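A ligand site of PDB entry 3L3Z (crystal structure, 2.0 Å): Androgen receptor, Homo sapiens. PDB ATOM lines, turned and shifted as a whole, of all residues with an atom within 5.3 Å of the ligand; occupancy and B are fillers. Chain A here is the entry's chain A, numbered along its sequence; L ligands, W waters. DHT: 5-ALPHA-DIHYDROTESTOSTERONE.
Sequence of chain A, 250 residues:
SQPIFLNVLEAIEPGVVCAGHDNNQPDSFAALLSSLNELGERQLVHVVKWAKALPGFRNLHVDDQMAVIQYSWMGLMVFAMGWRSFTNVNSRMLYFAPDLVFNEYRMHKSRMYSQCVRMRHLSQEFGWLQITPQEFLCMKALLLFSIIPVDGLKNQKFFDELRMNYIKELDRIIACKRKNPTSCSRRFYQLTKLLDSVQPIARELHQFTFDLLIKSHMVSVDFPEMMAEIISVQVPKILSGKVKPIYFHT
Leu 33 touches the ligand.
Leu 36 touches the ligand.
Leu 39 touches the ligand (CD2 to C2, 3.8 Å).
OE1 of Gln 43 touches C2 of the ligand, at 3.3 Å.
Met 74 touches the ligand (CE to C18, 3.7 Å).
Met 77 touches the ligand.
Met 81 touches the ligand.
CE1 of Phe 96 touches C5 of the ligand, at 3.7 Å.
Met 112 touches the ligand (SD to C15, 3.9 Å).
Phe 208 touches the ligand (CD1 to C16, 3.9 Å).
CE of Met 227 touches C12 of the ligand, at 3.8 Å.
Hydrophobic or aromatic side chains within 4 Å of the ligand: Leu 33, Leu 39, Met 74, Met 77, Met 81, Phe 96, Met 112, Phe 208 and Met 227.
Within 4 Å of the ligand: Leu 33, Leu 36, Asn 37, Leu 39, Gln 43, Met 74, Met 77, Met 81, Arg 84, Phe 96, Met 112, Phe 208, Thr 209 and Met 227.
Along chain A the residues within 4 Å of the ligand span positions 33 to 227.
The nearest printed residue that does not touch the ligand is Leu 212 (4.01 Å).
OD1 of Asn 37 lies within hydrogen-bond range of O17 of the ligand (2.8 Å).
The side-chain hydroxyl (OG1) of Thr 209 sits at hydrogen-bond distance from an oxygen (O17) of the ligand, 2.9 Å away.
The guanidinium group (NH2) of Arg 84 sits at hydrogen-bond distance from an oxygen (O3) of the ligand (3.0 Å).
The guanidinium group of Arg 84 sits close to the side-chain amide nitrogen of Gln 43 (3.5 Å).
NH2 of Arg 84 sits at hydrogen-bond distance from O of Phe 96, at 3.0 Å.
The side-chain sulfur (SD) of Met 77 sits close to the side-chain amide oxygen (OE1) of Gln 43, at 3.8 Å.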
ATOM      1  N   LEU A  33      -4.434  -0.501  -4.135  1.00  0.00           N
ATOM      2  CA  LEU A  33      -4.341   0.591  -5.101  1.00  0.00           C
ATOM      3  C   LEU A  33      -3.024   0.564  -5.840  1.00  0.00           C
ATOM      4  O   LEU A  33      -2.970   0.871  -7.020  1.00  0.00           O
ATOM      5  CB  LEU A  33      -4.595   1.946  -4.462  1.00  0.00           C
ATOM      6  CG  LEU A  33      -6.074   2.310  -4.405  1.00  0.00           C
ATOM      7  CD1 LEU A  33      -6.640   2.530  -5.782  1.00  0.00           C
ATOM      8  CD2 LEU A  33      -6.908   1.257  -3.649  1.00  0.00           C
ATOM      9  N   LEU A  36      -3.558  -1.953  -8.514  1.00  0.00           N
ATOM     10  CA  LEU A  36      -4.473  -1.473  -9.553  1.00  0.00           C
ATOM     11  C   LEU A  36      -3.682  -0.559 -10.465  1.00  0.00           C
ATOM     12  O   LEU A  36      -3.846  -0.628 -11.688  1.00  0.00           O
ATOM     13  CB  LEU A  36      -5.700  -0.740  -8.993  1.00  0.00           C
ATOM     14  CG  LEU A  36      -6.851  -1.581  -8.446  1.00  0.00           C
ATOM     15  CD1 LEU A  36      -7.862  -0.702  -7.791  1.00  0.00           C
ATOM     16  CD2 LEU A  36      -7.545  -2.458  -9.526  1.00  0.00           C
ATOM     17  N   ASN A  37      -2.825   0.296  -9.880  1.00  0.00           N
ATOM     18  CA  ASN A  37      -1.974   1.210 -10.664  1.00  0.00           C
ATOM     19  C   ASN A  37      -1.008   0.442 -11.576  1.00  0.00           C
ATOM     20  O   ASN A  37      -0.773   0.841 -12.703  1.00  0.00           O
ATOM     21  CB  ASN A  37      -1.165   2.127  -9.748  1.00  0.00           C
ATOM     22  CG  ASN A  37      -2.004   3.204  -9.086  1.00  0.00           C
ATOM     23  OD1 ASN A  37      -3.163   3.462  -9.466  1.00  0.00           O
ATOM     24  ND2 ASN A  37      -1.408   3.870  -8.069  1.00  0.00           N
ATOM     25  N   LEU A  39      -1.569  -2.624 -12.763  1.00  0.00           N
ATOM     26  CA  LEU A  39      -2.422  -3.212 -13.798  1.00  0.00           C
ATOM     27  C   LEU A  39      -2.773  -2.184 -14.872  1.00  0.00           C
ATOM     28  O   LEU A  39      -2.822  -2.485 -16.062  1.00  0.00           O
ATOM     29  CB  LEU A  39      -3.726  -3.688 -13.185  1.00  0.00           C
ATOM     30  CG  LEU A  39      -4.679  -4.371 -14.146  1.00  0.00           C
ATOM     31  CD1 LEU A  39      -4.040  -5.673 -14.687  1.00  0.00           C
ATOM     32  CD2 LEU A  39      -5.999  -4.668 -13.437  1.00  0.00           C
ATOM     33  N   GLY A  40      -3.030  -0.956 -14.442  1.00  0.00           N
ATOM     34  CA  GLY A  40      -3.311   0.107 -15.361  1.00  0.00           C
ATOM     35  C   GLY A  40      -2.132   0.326 -16.248  1.00  0.00           C
ATOM     36  O   GLY A  40      -2.288   0.512 -17.467  1.00  0.00           O
ATOM     37  N   GLN A  43      -1.867  -2.664 -18.634  1.00  0.00           N
ATOM     38  CA  GLN A  43      -2.933  -2.551 -19.580  1.00  0.00           C
ATOM     39  C   GLN A  43      -2.756  -1.399 -20.559  1.00  0.00           C
ATOM     40  O   GLN A  43      -3.163  -1.492 -21.725  1.00  0.00           O
ATOM     41  CB  GLN A  43      -4.296  -2.521 -18.880  1.00  0.00           C
ATOM     42  CG  GLN A  43      -4.739  -3.833 -18.347  1.00  0.00           C
ATOM     43  CD  GLN A  43      -6.168  -3.833 -17.997  1.00  0.00           C
ATOM     44  OE1 GLN A  43      -6.939  -2.971 -18.405  1.00  0.00           O
ATOM     45  NE2 GLN A  43      -6.565  -4.783 -17.191  1.00  0.00           N
ATOM     46  N   TRP A  73      -8.172   5.948 -22.095  1.00  0.00           N
ATOM     47  CA  TRP A  73      -7.807   4.675 -21.516  1.00  0.00           C
ATOM     48  C   TRP A  73      -8.709   4.273 -20.339  1.00  0.00           C
ATOM     49  O   TRP A  73      -9.060   3.103 -20.170  1.00  0.00           O
ATOM     50  CB  TRP A  73      -6.304   4.684 -21.118  1.00  0.00           C
ATOM     51  CG  TRP A  73      -5.961   5.719 -20.063  1.00  0.00           C
ATOM     52  CD1 TRP A  73      -5.454   6.931 -20.279  1.00  0.00           C
ATOM     53  CD2 TRP A  73      -6.019   5.545 -18.633  1.00  0.00           C
ATOM     54  NE1 TRP A  73      -5.244   7.578 -19.096  1.00  0.00           N
ATOM     55  CE2 TRP A  73      -5.577   6.747 -18.061  1.00  0.00           C
ATOM     56  CE3 TRP A  73      -6.429   4.513 -17.789  1.00  0.00           C
ATOM     57  CZ2 TRP A  73      -5.525   6.943 -16.673  1.00  0.00           C
ATOM     58  CZ3 TRP A  73      -6.353   4.697 -16.410  1.00  0.00           C
ATOM     59  CH2 TRP A  73      -5.917   5.907 -15.869  1.00  0.00           C
ATOM     60  N   MET A  74      -9.069   5.231 -19.478  1.00  0.00           N
ATOM     61  CA  MET A  74      -9.874   4.889 -18.326  1.00  0.00           C
ATOM     62  C   MET A  74     -11.174   4.245 -18.751  1.00  0.00           C
ATOM     63  O   MET A  74     -11.521   3.149 -18.265  1.00  0.00           O
ATOM     64  CB  MET A  74     -10.208   6.125 -17.469  1.00  0.00           C
ATOM     65  CG  MET A  74     -11.054   5.832 -16.244  1.00  0.00           C
ATOM     66  SD  MET A  74     -10.187   4.905 -14.980  1.00  0.00           S
ATOM     67  CE  MET A  74      -9.069   6.175 -14.283  1.00  0.00           C
ATOM     68  N   MET A  77     -10.605   0.732 -20.388  1.00  0.00           N
ATOM     69  CA  MET A  77     -10.286  -0.310 -19.413  1.00  0.00           C
ATOM     70  C   MET A  77     -11.452  -0.685 -18.517  1.00  0.00           C
ATOM     71  O   MET A  77     -11.595  -1.838 -18.201  1.00  0.00           O
ATOM     72  CB  MET A  77      -9.092   0.061 -18.536  1.00  0.00           C
ATOM     73  CG  MET A  77      -7.815   0.312 -19.306  1.00  0.00           C
ATOM     74  SD  MET A  77      -6.446   0.755 -18.266  1.00  0.00           S
ATOM     75  CE  MET A  77      -5.120   0.925 -19.531  1.00  0.00           C
ATOM     76  N   VAL A  78     -12.295   0.275 -18.131  1.00  0.00           N
ATOM     77  CA  VAL A  78     -13.498  -0.007 -17.342  1.00  0.00           C
ATOM     78  C   VAL A  78     -14.533  -0.817 -18.128  1.00  0.00           C
ATOM     79  O   VAL A  78     -15.149  -1.744 -17.616  1.00  0.00           O
ATOM     80  CB  VAL A  78     -14.160   1.292 -16.842  1.00  0.00           C
ATOM     81  CG1 VAL A  78     -15.535   1.003 -16.181  1.00  0.00           C
ATOM     82  CG2 VAL A  78     -13.225   1.954 -15.823  1.00  0.00           C
ATOM     83  N   MET A  81     -13.219  -4.326 -18.448  1.00  0.00           N
ATOM     84  CA  MET A  81     -13.229  -5.027 -17.148  1.00  0.00           C
ATOM     85  C   MET A  81     -14.659  -5.391 -16.807  1.00  0.00           C
ATOM     86  O   MET A  81     -14.926  -6.440 -16.231  1.00  0.00           O
ATOM     87  CB  MET A  81     -12.660  -4.132 -16.073  1.00  0.00           C
ATOM     88  CG  MET A  81     -12.530  -4.740 -14.721  1.00  0.00           C
ATOM     89  SD  MET A  81     -14.094  -4.613 -13.783  1.00  0.00           S
ATOM     90  CE  MET A  81     -14.061  -2.851 -13.462  1.00  0.00           C
ATOM     91  N   ARG A  84     -15.399  -8.613 -18.758  1.00  0.00           N
ATOM     92  CA  ARG A  84     -14.745  -9.738 -18.091  1.00  0.00           C
ATOM     93  C   ARG A  84     -15.465 -10.120 -16.851  1.00  0.00           C
ATOM     94  O   ARG A  84     -15.583 -11.299 -16.540  1.00  0.00           O
ATOM     95  CB  ARG A  84     -13.307  -9.384 -17.650  1.00  0.00           C
ATOM     96  CG  ARG A  84     -12.398  -9.125 -18.734  1.00  0.00           C
ATOM     97  CD  ARG A  84     -10.971  -9.197 -18.238  1.00  0.00           C
ATOM     98  NE  ARG A  84     -10.554  -8.077 -17.390  1.00  0.00           N
ATOM     99  CZ  ARG A  84     -10.257  -6.851 -17.832  1.00  0.00           C
ATOM    100  NH1 ARG A  84     -10.379  -6.536 -19.128  1.00  0.00           N
ATOM    101  NH2 ARG A  84      -9.839  -5.925 -16.980  1.00  0.00           N
ATOM    102  N   PHE A  96     -10.956  -7.442 -12.248  1.00  0.00           N
ATOM    103  CA  PHE A  96      -9.863  -6.577 -12.781  1.00  0.00           C
ATOM    104  C   PHE A  96      -8.800  -7.394 -13.499  1.00  0.00           C
ATOM    105  O   PHE A  96      -8.387  -7.046 -14.592  1.00  0.00           O
ATOM    106  CB  PHE A  96      -9.196  -5.788 -11.643  1.00  0.00           C
ATOM    107  CG  PHE A  96     -10.076  -4.763 -11.047  1.00  0.00           C
ATOM    108  CD1 PHE A  96     -10.414  -3.645 -11.752  1.00  0.00           C
ATOM    109  CD2 PHE A  96     -10.567  -4.916  -9.749  1.00  0.00           C
ATOM    110  CE1 PHE A  96     -11.253  -2.695 -11.211  1.00  0.00           C
ATOM    111  CE2 PHE A  96     -11.408  -3.959  -9.202  1.00  0.00           C
ATOM    112  CZ  PHE A  96     -11.731  -2.842  -9.933  1.00  0.00           C
ATOM    113  N   MET A 112     -13.030   3.033  -2.615  1.00  0.00           N
ATOM    114  CA  MET A 112     -13.817   3.471  -3.754  1.00  0.00           C
ATOM    115  C   MET A 112     -14.979   2.505  -3.963  1.00  0.00           C
ATOM    116  O   MET A 112     -15.243   2.037  -5.064  1.00  0.00           O
ATOM    117  CB  MET A 112     -12.932   3.657  -5.044  1.00  0.00           C
ATOM    118  CG  MET A 112     -12.014   2.570  -5.384  1.00  0.00           C
ATOM    119  SD  MET A 112     -11.249   2.832  -6.998  1.00  0.00           S
ATOM    120  CE  MET A 112     -11.169   1.161  -7.520  1.00  0.00           C
ATOM    121  N   MET A 119     -19.424   0.431 -11.311  1.00  0.00           N
ATOM    122  CA  MET A 119     -18.767  -0.461 -12.282  1.00  0.00           C
ATOM    123  C   MET A 119     -19.489  -1.806 -12.352  1.00  0.00           C
ATOM    124  O   MET A 119     -19.601  -2.415 -13.426  1.00  0.00           O
ATOM    125  CB  MET A 119     -17.263  -0.655 -11.936  1.00  0.00           C
ATOM    126  CG  MET A 119     -16.401   0.574 -12.259  1.00  0.00           C
ATOM    127  SD  MET A 119     -14.644   0.337 -12.082  1.00  0.00           S
ATOM    128  CE  MET A 119     -14.406   0.568 -10.321  1.00  0.00           C
ATOM    129  N   LEU A 205     -13.572   7.994 -11.495  1.00  0.00           N
ATOM    130  CA  LEU A 205     -12.314   7.297 -11.326  1.00  0.00           C
ATOM    131  C   LEU A 205     -11.171   8.268 -11.601  1.00  0.00           C
ATOM    132  O   LEU A 205     -10.159   8.245 -10.903  1.00  0.00           O
ATOM    133  CB  LEU A 205     -12.230   6.057 -12.225  1.00  0.00           C
ATOM    134  CG  LEU A 205     -13.242   4.971 -11.827  1.00  0.00           C
ATOM    135  CD1 LEU A 205     -13.355   3.846 -12.876  1.00  0.00           C
ATOM    136  CD2 LEU A 205     -12.928   4.419 -10.462  1.00  0.00           C
ATOM    137  N   PHE A 208     -10.889  10.422  -8.499  1.00  0.00           N
ATOM    138  CA  PHE A 208     -10.303   9.630  -7.461  1.00  0.00           C
ATOM    139  C   PHE A 208      -8.797   9.441  -7.661  1.00  0.00           C
ATOM    140  O   PHE A 208      -8.027   9.659  -6.745  1.00  0.00           O
ATOM    141  CB  PHE A 208     -10.971   8.260  -7.409  1.00  0.00           C
ATOM    142  CG  PHE A 208     -10.606   7.444  -6.201  1.00  0.00           C
ATOM    143  CD1 PHE A 208      -9.509   6.601  -6.211  1.00  0.00           C
ATOM    144  CD2 PHE A 208     -11.373   7.491  -5.043  1.00  0.00           C
ATOM    145  CE1 PHE A 208      -9.213   5.822  -5.116  1.00  0.00           C
ATOM    146  CE2 PHE A 208     -11.032   6.715  -3.918  1.00  0.00           C
ATOM    147  CZ  PHE A 208      -9.952   5.900  -3.971  1.00  0.00           C
ATOM    148  N   THR A 209      -8.402   8.999  -8.847  1.00  0.00           N
ATOM    149  CA  THR A 209      -6.969   8.717  -9.070  1.00  0.00           C
ATOM    150  C   THR A 209      -6.122  10.000  -9.003  1.00  0.00           C
ATOM    151  O   THR A 209      -4.977   9.964  -8.582  1.00  0.00           O
ATOM    152  CB  THR A 209      -6.735   7.957 -10.389  1.00  0.00           C
ATOM    153  OG1 THR A 209      -5.398   7.491 -10.418  1.00  0.00           O
ATOM    154  CG2 THR A 209      -6.989   8.801 -11.608  1.00  0.00           C
ATOM    155  N   LEU A 212      -5.694  10.775  -5.438  1.00  0.00           N
ATOM    156  CA  LEU A 212      -4.822   9.755  -4.880  1.00  0.00           C
ATOM    157  C   LEU A 212      -3.374  10.071  -5.218  1.00  0.00           C
ATOM    158  O   LEU A 212      -2.487   9.968  -4.373  1.00  0.00           O
ATOM    159  CB  LEU A 212      -5.267   8.360  -5.310  1.00  0.00           C
ATOM    160  CG  LEU A 212      -4.414   7.213  -4.812  1.00  0.00           C
ATOM    161  CD1 LEU A 212      -4.412   7.181  -3.272  1.00  0.00           C
ATOM    162  CD2 LEU A 212      -4.894   5.908  -5.363  1.00  0.00           C
ATOM    163  N   PHE A 223       2.734   4.882  -7.945  1.00  0.00           N
ATOM    164  CA  PHE A 223       2.217   5.103  -9.306  1.00  0.00           C
ATOM    165  C   PHE A 223       3.345   4.841 -10.269  1.00  0.00           C
ATOM    166  O   PHE A 223       4.426   5.449 -10.144  1.00  0.00           O
ATOM    167  CB  PHE A 223       1.720   6.542  -9.468  1.00  0.00           C
ATOM    168  CG  PHE A 223       0.324   6.755  -8.981  1.00  0.00           C
ATOM    169  CD1 PHE A 223       0.039   6.850  -7.625  1.00  0.00           C
ATOM    170  CD2 PHE A 223      -0.707   6.794  -9.881  1.00  0.00           C
ATOM    171  CE1 PHE A 223      -1.282   7.030  -7.184  1.00  0.00           C
ATOM    172  CE2 PHE A 223      -2.058   6.970  -9.446  1.00  0.00           C
ATOM    173  CZ  PHE A 223      -2.326   7.107  -8.107  1.00  0.00           C
ATOM    174  N   MET A 227       1.527   6.050 -15.810  1.00  0.00           N
ATOM    175  CA  MET A 227       0.310   6.459 -15.117  1.00  0.00           C
ATOM    176  C   MET A 227       0.522   7.794 -14.420  1.00  0.00           C
ATOM    177  O   MET A 227      -0.291   8.681 -14.548  1.00  0.00           O
ATOM    178  CB  MET A 227      -0.125   5.400 -14.108  1.00  0.00           C
ATOM    179  CG  MET A 227      -0.509   4.045 -14.691  1.00  0.00           C
ATOM    180  SD  MET A 227      -2.138   4.114 -15.438  1.00  0.00           S
ATOM    181  CE  MET A 227      -3.117   3.721 -14.008  1.00  0.00           C
HETATM  182  C1  DHT L   1      -7.104  -0.887 -14.153  1.00  0.00           C
HETATM  183  C2  DHT L   1      -7.517  -1.788 -15.349  1.00  0.00           C
HETATM  184  C3  DHT L   1      -8.966  -2.257 -15.151  1.00  0.00           C
HETATM  185  O3  DHT L   1      -9.281  -3.438 -15.352  1.00  0.00           O
HETATM  186  C4  DHT L   1      -9.971  -1.218 -14.676  1.00  0.00           C
HETATM  187  C5  DHT L   1      -9.461  -0.393 -13.494  1.00  0.00           C
HETATM  188  C6  DHT L   1     -10.482   0.654 -13.002  1.00  0.00           C
HETATM  189  C7  DHT L   1      -9.992   1.388 -11.739  1.00  0.00           C
HETATM  190  C8  DHT L   1      -8.606   2.037 -11.981  1.00  0.00           C
HETATM  191  C9  DHT L   1      -7.582   0.994 -12.495  1.00  0.00           C
HETATM  192  C10 DHT L   1      -8.061   0.247 -13.754  1.00  0.00           C
HETATM  193  C11 DHT L   1      -6.188   1.647 -12.671  1.00  0.00           C
HETATM  194  C12 DHT L   1      -5.650   2.471 -11.476  1.00  0.00           C
HETATM  195  C13 DHT L   1      -6.684   3.450 -10.897  1.00  0.00           C
HETATM  196  C14 DHT L   1      -8.013   2.719 -10.727  1.00  0.00           C
HETATM  197  C15 DHT L   1      -8.888   3.733  -9.976  1.00  0.00           C
HETATM  198  C16 DHT L   1      -7.923   4.335  -8.950  1.00  0.00           C
HETATM  199  C17 DHT L   1      -6.521   3.885  -9.425  1.00  0.00           C
HETATM  200  O17 DHT L   1      -5.557   4.900  -9.190  1.00  0.00           O
HETATM  201  C18 DHT L   1      -6.724   4.676 -11.820  1.00  0.00           C
HETATM  202  C19 DHT L   1      -8.082   1.254 -14.927  1.00  0.00           C
HETATM  203  O   HOH W   1      -9.537  -3.615 -18.585  1.00  0.00           O
